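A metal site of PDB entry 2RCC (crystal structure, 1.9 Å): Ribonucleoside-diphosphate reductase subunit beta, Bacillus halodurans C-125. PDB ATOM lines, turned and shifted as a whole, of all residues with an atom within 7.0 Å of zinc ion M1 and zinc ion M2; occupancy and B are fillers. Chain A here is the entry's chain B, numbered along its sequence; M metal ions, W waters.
OD1 of Asp 182 sits close to OE1 of Glu 186, 2.6 Å away.
OE2 of Glu 186 lies close to NE2 of Gln 92, at 3.3 Å.
A ring nitrogen (NE2) of His 223 is in hydrogen-bond range of the side-chain amide oxygen of Gln 118 (2.6 Å).
OH of Tyr 126 is in hydrogen-bond range of OD2 of Asp 89 (3.0 Å).
A ring nitrogen (NE2) of His 122 lies within hydrogen-bond range of the side-chain carboxylate (OD2) of Asp 219, at 2.8 Å.
Within 4 Å of zinc ion M1: Glu 119, Glu 186, Glu 220 and His 223.
Within 4 Å of zinc ion M2: Asp 89, Glu 119, His 122 and Glu 220.
Along chain A the residues within 4 Å of zinc ion M2 span positions 89 to 220.
OE2 of Glu 186 is bound to zinc ion M1.
Water W2 is bound to zinc ion M1 (2.0 Å).
Zinc ion M1 is bound by OE2 of Glu 119, 2.1 Å away.
OE1 of Glu 220 binds zinc ion M1, at 2.1 Å.
ND1 of His 223 is bound to zinc ion M1, at 2.3 Å.
Water W3 is bound to zinc ion M1 (2.3 Å).
Zinc ion M1 has six donor atoms within binding distance.
Zinc ion M2 is bound by water W1 (2.1 Å), ND1 of His 122 (2.1 Å), water W2 (2.2 Å) and OE1 of Glu 119 (2.2 Å).
Slightly farther from zinc ion M2 lies the side-chain carboxylate (OD1) of Asp 89 (2.7 Å).
Slightly farther from zinc ion M2 lies the side-chain carboxylate (OD2) of Asp 89 (2.8 Å).
Water W3 bridges the side-chain carboxylate of Asp 89 (2.8 Å) and the side-chain carboxylate of Glu 220 (3.0 Å).
Water W1 bridges the side-chain carboxylate (OE2) of Glu 220 (2.9 Å) and the side-chain carboxylate (OD2) of Asp 89 (3.1 Å).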
ATOM      1  N   LEU A  85     -20.079  12.080   2.703  1.00  0.00           N
ATOM      2  CA  LEU A  85     -19.728  13.467   2.986  1.00  0.00           C
ATOM      3  C   LEU A  85     -20.437  14.432   2.037  1.00  0.00           C
ATOM      4  O   LEU A  85     -20.859  15.493   2.483  1.00  0.00           O
ATOM      5  CB  LEU A  85     -18.207  13.681   2.961  1.00  0.00           C
ATOM      6  CG  LEU A  85     -17.432  12.830   3.983  1.00  0.00           C
ATOM      7  CD1 LEU A  85     -15.957  13.205   4.007  1.00  0.00           C
ATOM      8  CD2 LEU A  85     -18.056  12.866   5.404  1.00  0.00           C
ATOM      9  N   LEU A  88     -23.994  14.635   3.211  1.00  0.00           N
ATOM     10  CA  LEU A  88     -24.056  15.461   4.422  1.00  0.00           C
ATOM     11  C   LEU A  88     -23.823  16.943   4.146  1.00  0.00           C
ATOM     12  O   LEU A  88     -24.564  17.769   4.663  1.00  0.00           O
ATOM     13  CB  LEU A  88     -23.084  14.962   5.498  1.00  0.00           C
ATOM     14  CG  LEU A  88     -23.385  13.583   6.084  1.00  0.00           C
ATOM     15  CD1 LEU A  88     -22.319  13.212   7.014  1.00  0.00           C
ATOM     16  CD2 LEU A  88     -24.810  13.553   6.759  1.00  0.00           C
ATOM     17  N   ASP A  89     -22.794  17.287   3.394  1.00  0.00           N
ATOM     18  CA  ASP A  89     -22.574  18.739   3.064  1.00  0.00           C
ATOM     19  C   ASP A  89     -23.602  19.355   2.097  1.00  0.00           C
ATOM     20  O   ASP A  89     -23.819  20.547   2.158  1.00  0.00           O
ATOM     21  CB  ASP A  89     -21.171  19.055   2.608  1.00  0.00           C
ATOM     22  CG  ASP A  89     -20.208  19.294   3.763  1.00  0.00           C
ATOM     23  OD1 ASP A  89     -20.648  19.635   4.912  1.00  0.00           O
ATOM     24  OD2 ASP A  89     -19.012  19.056   3.518  1.00  0.00           O
ATOM     25  N   GLN A  92     -26.366  20.026   4.540  1.00  0.00           N
ATOM     26  CA  GLN A  92     -25.886  21.073   5.453  1.00  0.00           C
ATOM     27  C   GLN A  92     -25.849  22.466   4.814  1.00  0.00           C
ATOM     28  O   GLN A  92     -26.086  23.493   5.483  1.00  0.00           O
ATOM     29  CB  GLN A  92     -24.494  20.680   5.985  1.00  0.00           C
ATOM     30  CG  GLN A  92     -23.876  21.602   7.016  1.00  0.00           C
ATOM     31  CD  GLN A  92     -24.629  21.669   8.309  1.00  0.00           C
ATOM     32  OE1 GLN A  92     -25.552  20.917   8.547  1.00  0.00           O
ATOM     33  NE2 GLN A  92     -24.218  22.592   9.173  1.00  0.00           N
ATOM     34  N   LEU A 115     -20.774  30.307   6.937  1.00  0.00           N
ATOM     35  CA  LEU A 115     -20.725  28.853   7.146  1.00  0.00           C
ATOM     36  C   LEU A 115     -21.419  28.144   5.970  1.00  0.00           C
ATOM     37  O   LEU A 115     -20.844  27.219   5.449  1.00  0.00           O
ATOM     38  CB  LEU A 115     -21.366  28.433   8.488  1.00  0.00           C
ATOM     39  CG  LEU A 115     -21.436  26.938   8.877  1.00  0.00           C
ATOM     40  CD1 LEU A 115     -21.443  26.789  10.413  1.00  0.00           C
ATOM     41  CD2 LEU A 115     -22.635  26.164   8.240  1.00  0.00           C
ATOM     42  N   GLN A 118     -19.215  28.175   2.995  1.00  0.00           N
ATOM     43  CA  GLN A 118     -18.092  27.178   3.142  1.00  0.00           C
ATOM     44  C   GLN A 118     -18.531  25.742   2.808  1.00  0.00           C
ATOM     45  O   GLN A 118     -17.779  24.962   2.178  1.00  0.00           O
ATOM     46  CB  GLN A 118     -17.466  27.273   4.523  1.00  0.00           C
ATOM     47  CG  GLN A 118     -16.776  28.587   4.752  1.00  0.00           C
ATOM     48  CD  GLN A 118     -16.044  28.669   6.054  1.00  0.00           C
ATOM     49  OE1 GLN A 118     -16.329  27.961   7.005  1.00  0.00           O
ATOM     50  NE2 GLN A 118     -15.091  29.579   6.115  1.00  0.00           N
ATOM     51  N   GLU A 119     -19.781  25.429   3.152  1.00  0.00           N
ATOM     52  CA  GLU A 119     -20.411  24.152   2.851  1.00  0.00           C
ATOM     53  C   GLU A 119     -20.628  23.965   1.354  1.00  0.00           C
ATOM     54  O   GLU A 119     -20.423  22.867   0.848  1.00  0.00           O
ATOM     55  CB  GLU A 119     -21.737  23.980   3.584  1.00  0.00           C
ATOM     56  CG  GLU A 119     -21.750  24.038   5.120  1.00  0.00           C
ATOM     57  CD  GLU A 119     -20.824  23.060   5.802  1.00  0.00           C
ATOM     58  OE1 GLU A 119     -19.994  22.410   5.176  1.00  0.00           O
ATOM     59  OE2 GLU A 119     -20.899  22.980   7.022  1.00  0.00           O
ATOM     60  N   VAL A 120     -20.983  25.040   0.646  1.00  0.00           N
ATOM     61  CA  VAL A 120     -21.057  24.988  -0.817  1.00  0.00           C
ATOM     62  C   VAL A 120     -19.676  24.545  -1.400  1.00  0.00           C
ATOM     63  O   VAL A 120     -19.625  23.622  -2.235  1.00  0.00           O
ATOM     64  CB  VAL A 120     -21.498  26.337  -1.465  1.00  0.00           C
ATOM     65  CG1 VAL A 120     -21.342  26.274  -2.998  1.00  0.00           C
ATOM     66  CG2 VAL A 120     -22.926  26.716  -1.078  1.00  0.00           C
ATOM     67  N   HIS A 122     -17.103  22.975   0.236  1.00  0.00           N
ATOM     68  CA  HIS A 122     -16.805  21.617   0.723  1.00  0.00           C
ATOM     69  C   HIS A 122     -17.506  20.622  -0.146  1.00  0.00           C
ATOM     70  O   HIS A 122     -16.881  19.695  -0.597  1.00  0.00           O
ATOM     71  CB  HIS A 122     -17.298  21.421   2.129  1.00  0.00           C
ATOM     72  CG  HIS A 122     -16.568  22.223   3.161  1.00  0.00           C
ATOM     73  ND1 HIS A 122     -16.793  22.057   4.517  1.00  0.00           N
ATOM     74  CD2 HIS A 122     -15.638  23.187   3.051  1.00  0.00           C
ATOM     75  CE1 HIS A 122     -16.053  22.918   5.188  1.00  0.00           C
ATOM     76  NE2 HIS A 122     -15.324  23.610   4.328  1.00  0.00           N
ATOM     77  N   ASN A 123     -18.807  20.815  -0.393  1.00  0.00           N
ATOM     78  CA  ASN A 123     -19.574  19.884  -1.202  1.00  0.00           C
ATOM     79  C   ASN A 123     -19.010  19.806  -2.616  1.00  0.00           C
ATOM     80  O   ASN A 123     -18.815  18.722  -3.162  1.00  0.00           O
ATOM     81  CB  ASN A 123     -21.058  20.214  -1.219  1.00  0.00           C
ATOM     82  CG  ASN A 123     -21.847  19.248  -2.054  1.00  0.00           C
ATOM     83  OD1 ASN A 123     -21.957  18.077  -1.699  1.00  0.00           O
ATOM     84  ND2 ASN A 123     -22.386  19.710  -3.151  1.00  0.00           N
ATOM     85  N   TYR A 126     -15.908  17.670  -3.240  1.00  0.00           N
ATOM     86  CA  TYR A 126     -16.098  16.195  -3.414  1.00  0.00           C
ATOM     87  C   TYR A 126     -16.352  15.838  -4.871  1.00  0.00           C
ATOM     88  O   TYR A 126     -15.890  14.790  -5.321  1.00  0.00           O
ATOM     89  CB  TYR A 126     -17.186  15.584  -2.494  1.00  0.00           C
ATOM     90  CG  TYR A 126     -17.037  15.992  -1.089  1.00  0.00           C
ATOM     91  CD1 TYR A 126     -15.842  15.802  -0.400  1.00  0.00           C
ATOM     92  CD2 TYR A 126     -18.086  16.568  -0.409  1.00  0.00           C
ATOM     93  CE1 TYR A 126     -15.720  16.206   0.895  1.00  0.00           C
ATOM     94  CE2 TYR A 126     -17.960  16.960   0.867  1.00  0.00           C
ATOM     95  CZ  TYR A 126     -16.788  16.794   1.511  1.00  0.00           C
ATOM     96  OH  TYR A 126     -16.708  17.238   2.778  1.00  0.00           O
ATOM     97  N   ASP A 182     -26.929  19.079  14.096  1.00  0.00           N
ATOM     98  CA  ASP A 182     -25.856  19.762  13.400  1.00  0.00           C
ATOM     99  C   ASP A 182     -24.494  19.402  13.973  1.00  0.00           C
ATOM    100  O   ASP A 182     -23.573  19.101  13.209  1.00  0.00           O
ATOM    101  CB  ASP A 182     -26.034  21.267  13.416  1.00  0.00           C
ATOM    102  CG  ASP A 182     -24.947  21.949  12.686  1.00  0.00           C
ATOM    103  OD1 ASP A 182     -23.820  22.077  13.265  1.00  0.00           O
ATOM    104  OD2 ASP A 182     -25.216  22.287  11.525  1.00  0.00           O
ATOM    105  N   LEU A 185     -23.565  16.032  12.846  1.00  0.00           N
ATOM    106  CA  LEU A 185     -23.124  15.988  11.442  1.00  0.00           C
ATOM    107  C   LEU A 185     -21.716  16.545  11.273  1.00  0.00           C
ATOM    108  O   LEU A 185     -20.862  15.876  10.722  1.00  0.00           O
ATOM    109  CB  LEU A 185     -24.152  16.712  10.552  1.00  0.00           C
ATOM    110  CG  LEU A 185     -24.046  16.781   9.020  1.00  0.00           C
ATOM    111  CD1 LEU A 185     -25.395  17.073   8.437  1.00  0.00           C
ATOM    112  CD2 LEU A 185     -22.998  17.808   8.592  1.00  0.00           C
ATOM    113  N   GLU A 186     -21.496  17.743  11.802  1.00  0.00           N
ATOM    114  CA  GLU A 186     -20.223  18.448  11.650  1.00  0.00           C
ATOM    115  C   GLU A 186     -19.128  18.005  12.570  1.00  0.00           C
ATOM    116  O   GLU A 186     -17.970  17.919  12.171  1.00  0.00           O
ATOM    117  CB  GLU A 186     -20.445  19.958  11.868  1.00  0.00           C
ATOM    118  CG  GLU A 186     -21.426  20.525  10.859  1.00  0.00           C
ATOM    119  CD  GLU A 186     -21.382  22.047  10.790  1.00  0.00           C
ATOM    120  OE1 GLU A 186     -21.819  22.765  11.719  1.00  0.00           O
ATOM    121  OE2 GLU A 186     -20.941  22.534   9.771  1.00  0.00           O
ATOM    122  N   GLY A 187     -19.491  17.763  13.814  1.00  0.00           N
ATOM    123  CA  GLY A 187     -18.543  17.421  14.881  1.00  0.00           C
ATOM    124  C   GLY A 187     -18.284  15.971  15.171  1.00  0.00           C
ATOM    125  O   GLY A 187     -17.329  15.710  15.856  1.00  0.00           O
ATOM    126  N   PHE A 190     -18.255  14.041  10.364  1.00  0.00           N
ATOM    127  CA  PHE A 190     -17.099  14.502   9.593  1.00  0.00           C
ATOM    128  C   PHE A 190     -15.813  14.096  10.277  1.00  0.00           C
ATOM    129  O   PHE A 190     -14.869  13.671   9.610  1.00  0.00           O
ATOM    130  CB  PHE A 190     -17.178  16.013   9.254  1.00  0.00           C
ATOM    131  CG  PHE A 190     -17.880  16.276   7.956  1.00  0.00           C
ATOM    132  CD1 PHE A 190     -19.265  16.386   7.893  1.00  0.00           C
ATOM    133  CD2 PHE A 190     -17.161  16.259   6.769  1.00  0.00           C
ATOM    134  CE1 PHE A 190     -19.914  16.565   6.690  1.00  0.00           C
ATOM    135  CE2 PHE A 190     -17.788  16.400   5.553  1.00  0.00           C
ATOM    136  CZ  PHE A 190     -19.180  16.552   5.516  1.00  0.00           C
ATOM    137  N   PHE A 194     -12.691  12.071   8.770  1.00  0.00           N
ATOM    138  CA  PHE A 194     -11.320  12.592   8.627  1.00  0.00           C
ATOM    139  C   PHE A 194     -10.250  11.596   8.987  1.00  0.00           C
ATOM    140  O   PHE A 194      -9.210  11.589   8.330  1.00  0.00           O
ATOM    141  CB  PHE A 194     -11.059  13.893   9.428  1.00  0.00           C
ATOM    142  CG  PHE A 194     -12.011  15.043   9.144  1.00  0.00           C
ATOM    143  CD1 PHE A 194     -12.542  15.262   7.894  1.00  0.00           C
ATOM    144  CD2 PHE A 194     -12.324  15.938  10.150  1.00  0.00           C
ATOM    145  CE1 PHE A 194     -13.408  16.341   7.642  1.00  0.00           C
ATOM    146  CE2 PHE A 194     -13.198  17.014   9.910  1.00  0.00           C
ATOM    147  CZ  PHE A 194     -13.716  17.223   8.648  1.00  0.00           C
ATOM    148  N   ILE A 216     -10.834  21.344   4.998  1.00  0.00           N
ATOM    149  CA  ILE A 216     -12.259  21.157   5.402  1.00  0.00           C
ATOM    150  C   ILE A 216     -12.394  21.055   6.949  1.00  0.00           C
ATOM    151  O   ILE A 216     -13.304  21.636   7.552  1.00  0.00           O
ATOM    152  CB  ILE A 216     -12.855  19.889   4.727  1.00  0.00           C
ATOM    153  CG1 ILE A 216     -12.995  20.093   3.208  1.00  0.00           C
ATOM    154  CG2 ILE A 216     -14.172  19.510   5.343  1.00  0.00           C
ATOM    155  CD1 ILE A 216     -13.321  18.792   2.405  1.00  0.00           C
ATOM    156  N   ASP A 219     -12.048  24.368   8.701  1.00  0.00           N
ATOM    157  CA  ASP A 219     -13.370  25.080   8.641  1.00  0.00           C
ATOM    158  C   ASP A 219     -14.372  24.472   9.616  1.00  0.00           C
ATOM    159  O   ASP A 219     -15.136  25.200  10.312  1.00  0.00           O
ATOM    160  CB  ASP A 219     -13.977  25.036   7.253  1.00  0.00           C
ATOM    161  CG  ASP A 219     -13.212  25.822   6.231  1.00  0.00           C
ATOM    162  OD1 ASP A 219     -12.425  26.715   6.587  1.00  0.00           O
ATOM    163  OD2 ASP A 219     -13.437  25.512   5.050  1.00  0.00           O
ATOM    164  N   GLU A 220     -14.416  23.146   9.634  1.00  0.00           N
ATOM    165  CA  GLU A 220     -15.318  22.391  10.486  1.00  0.00           C
ATOM    166  C   GLU A 220     -15.199  22.725  11.973  1.00  0.00           C
ATOM    167  O   GLU A 220     -16.218  22.835  12.648  1.00  0.00           O
ATOM    168  CB  GLU A 220     -15.129  20.892  10.291  1.00  0.00           C
ATOM    169  CG  GLU A 220     -16.301  20.067  10.670  1.00  0.00           C
ATOM    170  CD  GLU A 220     -17.450  20.184   9.670  1.00  0.00           C
ATOM    171  OE1 GLU A 220     -18.268  21.133   9.765  1.00  0.00           O
ATOM    172  OE2 GLU A 220     -17.569  19.304   8.805  1.00  0.00           O
ATOM    173  N   GLN A 221     -13.969  22.893  12.441  1.00  0.00           N
ATOM    174  CA  GLN A 221     -13.712  23.262  13.841  1.00  0.00           C
ATOM    175  C   GLN A 221     -14.475  24.518  14.250  1.00  0.00           C
ATOM    176  O   GLN A 221     -15.109  24.555  15.307  1.00  0.00           O
ATOM    177  CB  GLN A 221     -12.200  23.445  14.051  1.00  0.00           C
ATOM    178  CG  GLN A 221     -11.813  23.712  15.489  1.00  0.00           C
ATOM    179  CD  GLN A 221     -10.313  23.872  15.657  1.00  0.00           C
ATOM    180  OE1 GLN A 221      -9.629  24.423  14.787  1.00  0.00           O
ATOM    181  NE2 GLN A 221      -9.803  23.414  16.788  1.00  0.00           N
ATOM    182  N   HIS A 223     -17.114  25.781  12.525  1.00  0.00           N
ATOM    183  CA  HIS A 223     -18.560  25.503  12.397  1.00  0.00           C
ATOM    184  C   HIS A 223     -19.164  24.947  13.726  1.00  0.00           C
ATOM    185  O   HIS A 223     -20.247  25.390  14.183  1.00  0.00           O
ATOM    186  CB  HIS A 223     -18.812  24.496  11.284  1.00  0.00           C
ATOM    187  CG  HIS A 223     -18.453  24.982   9.910  1.00  0.00           C
ATOM    188  ND1 HIS A 223     -18.733  24.250   8.766  1.00  0.00           N
ATOM    189  CD2 HIS A 223     -17.890  26.140   9.484  1.00  0.00           C
ATOM    190  CE1 HIS A 223     -18.348  24.944   7.712  1.00  0.00           C
ATOM    191  NE2 HIS A 223     -17.814  26.079   8.117  1.00  0.00           N
ATOM    192  N   VAL A 224     -18.446  24.010  14.341  1.00  0.00           N
ATOM    193  CA  VAL A 224     -18.836  23.371  15.595  1.00  0.00           C
ATOM    194  C   VAL A 224     -18.791  24.422  16.707  1.00  0.00           C
ATOM    195  O   VAL A 224     -19.702  24.501  17.504  1.00  0.00           O
ATOM    196  CB  VAL A 224     -17.960  22.142  15.937  1.00  0.00           C
ATOM    197  CG1 VAL A 224     -18.240  21.687  17.349  1.00  0.00           C
ATOM    198  CG2 VAL A 224     -18.205  21.041  14.962  1.00  0.00           C
ATOM    199  N   PHE A 227     -22.001  26.698  16.139  1.00  0.00           N
ATOM    200  CA  PHE A 227     -23.231  26.003  16.495  1.00  0.00           C
ATOM    201  C   PHE A 227     -23.369  25.710  17.984  1.00  0.00           C
ATOM    202  O   PHE A 227     -24.451  25.925  18.537  1.00  0.00           O
ATOM    203  CB  PHE A 227     -23.439  24.745  15.627  1.00  0.00           C
ATOM    204  CG  PHE A 227     -24.210  25.022  14.346  1.00  0.00           C
ATOM    205  CD1 PHE A 227     -25.586  25.218  14.405  1.00  0.00           C
ATOM    206  CD2 PHE A 227     -23.580  25.060  13.120  1.00  0.00           C
ATOM    207  CE1 PHE A 227     -26.316  25.464  13.279  1.00  0.00           C
ATOM    208  CE2 PHE A 227     -24.312  25.290  11.970  1.00  0.00           C
ATOM    209  CZ  PHE A 227     -25.672  25.499  12.053  1.00  0.00           C
HETATM  210 ZN    ZN M   1     -19.601  22.161   8.428  1.00  0.00          ZN
HETATM  211 ZN    ZN M   2     -18.371  20.951   5.453  1.00  0.00          ZN
HETATM  212  O   HOH W   1     -17.120  19.315   5.947  1.00  0.00           O
HETATM  213  O   HOH W   2     -17.969  21.723   7.447  1.00  0.00           O
HETATM  214  O   HOH W   3     -20.253  20.082   7.668  1.00  0.00           O
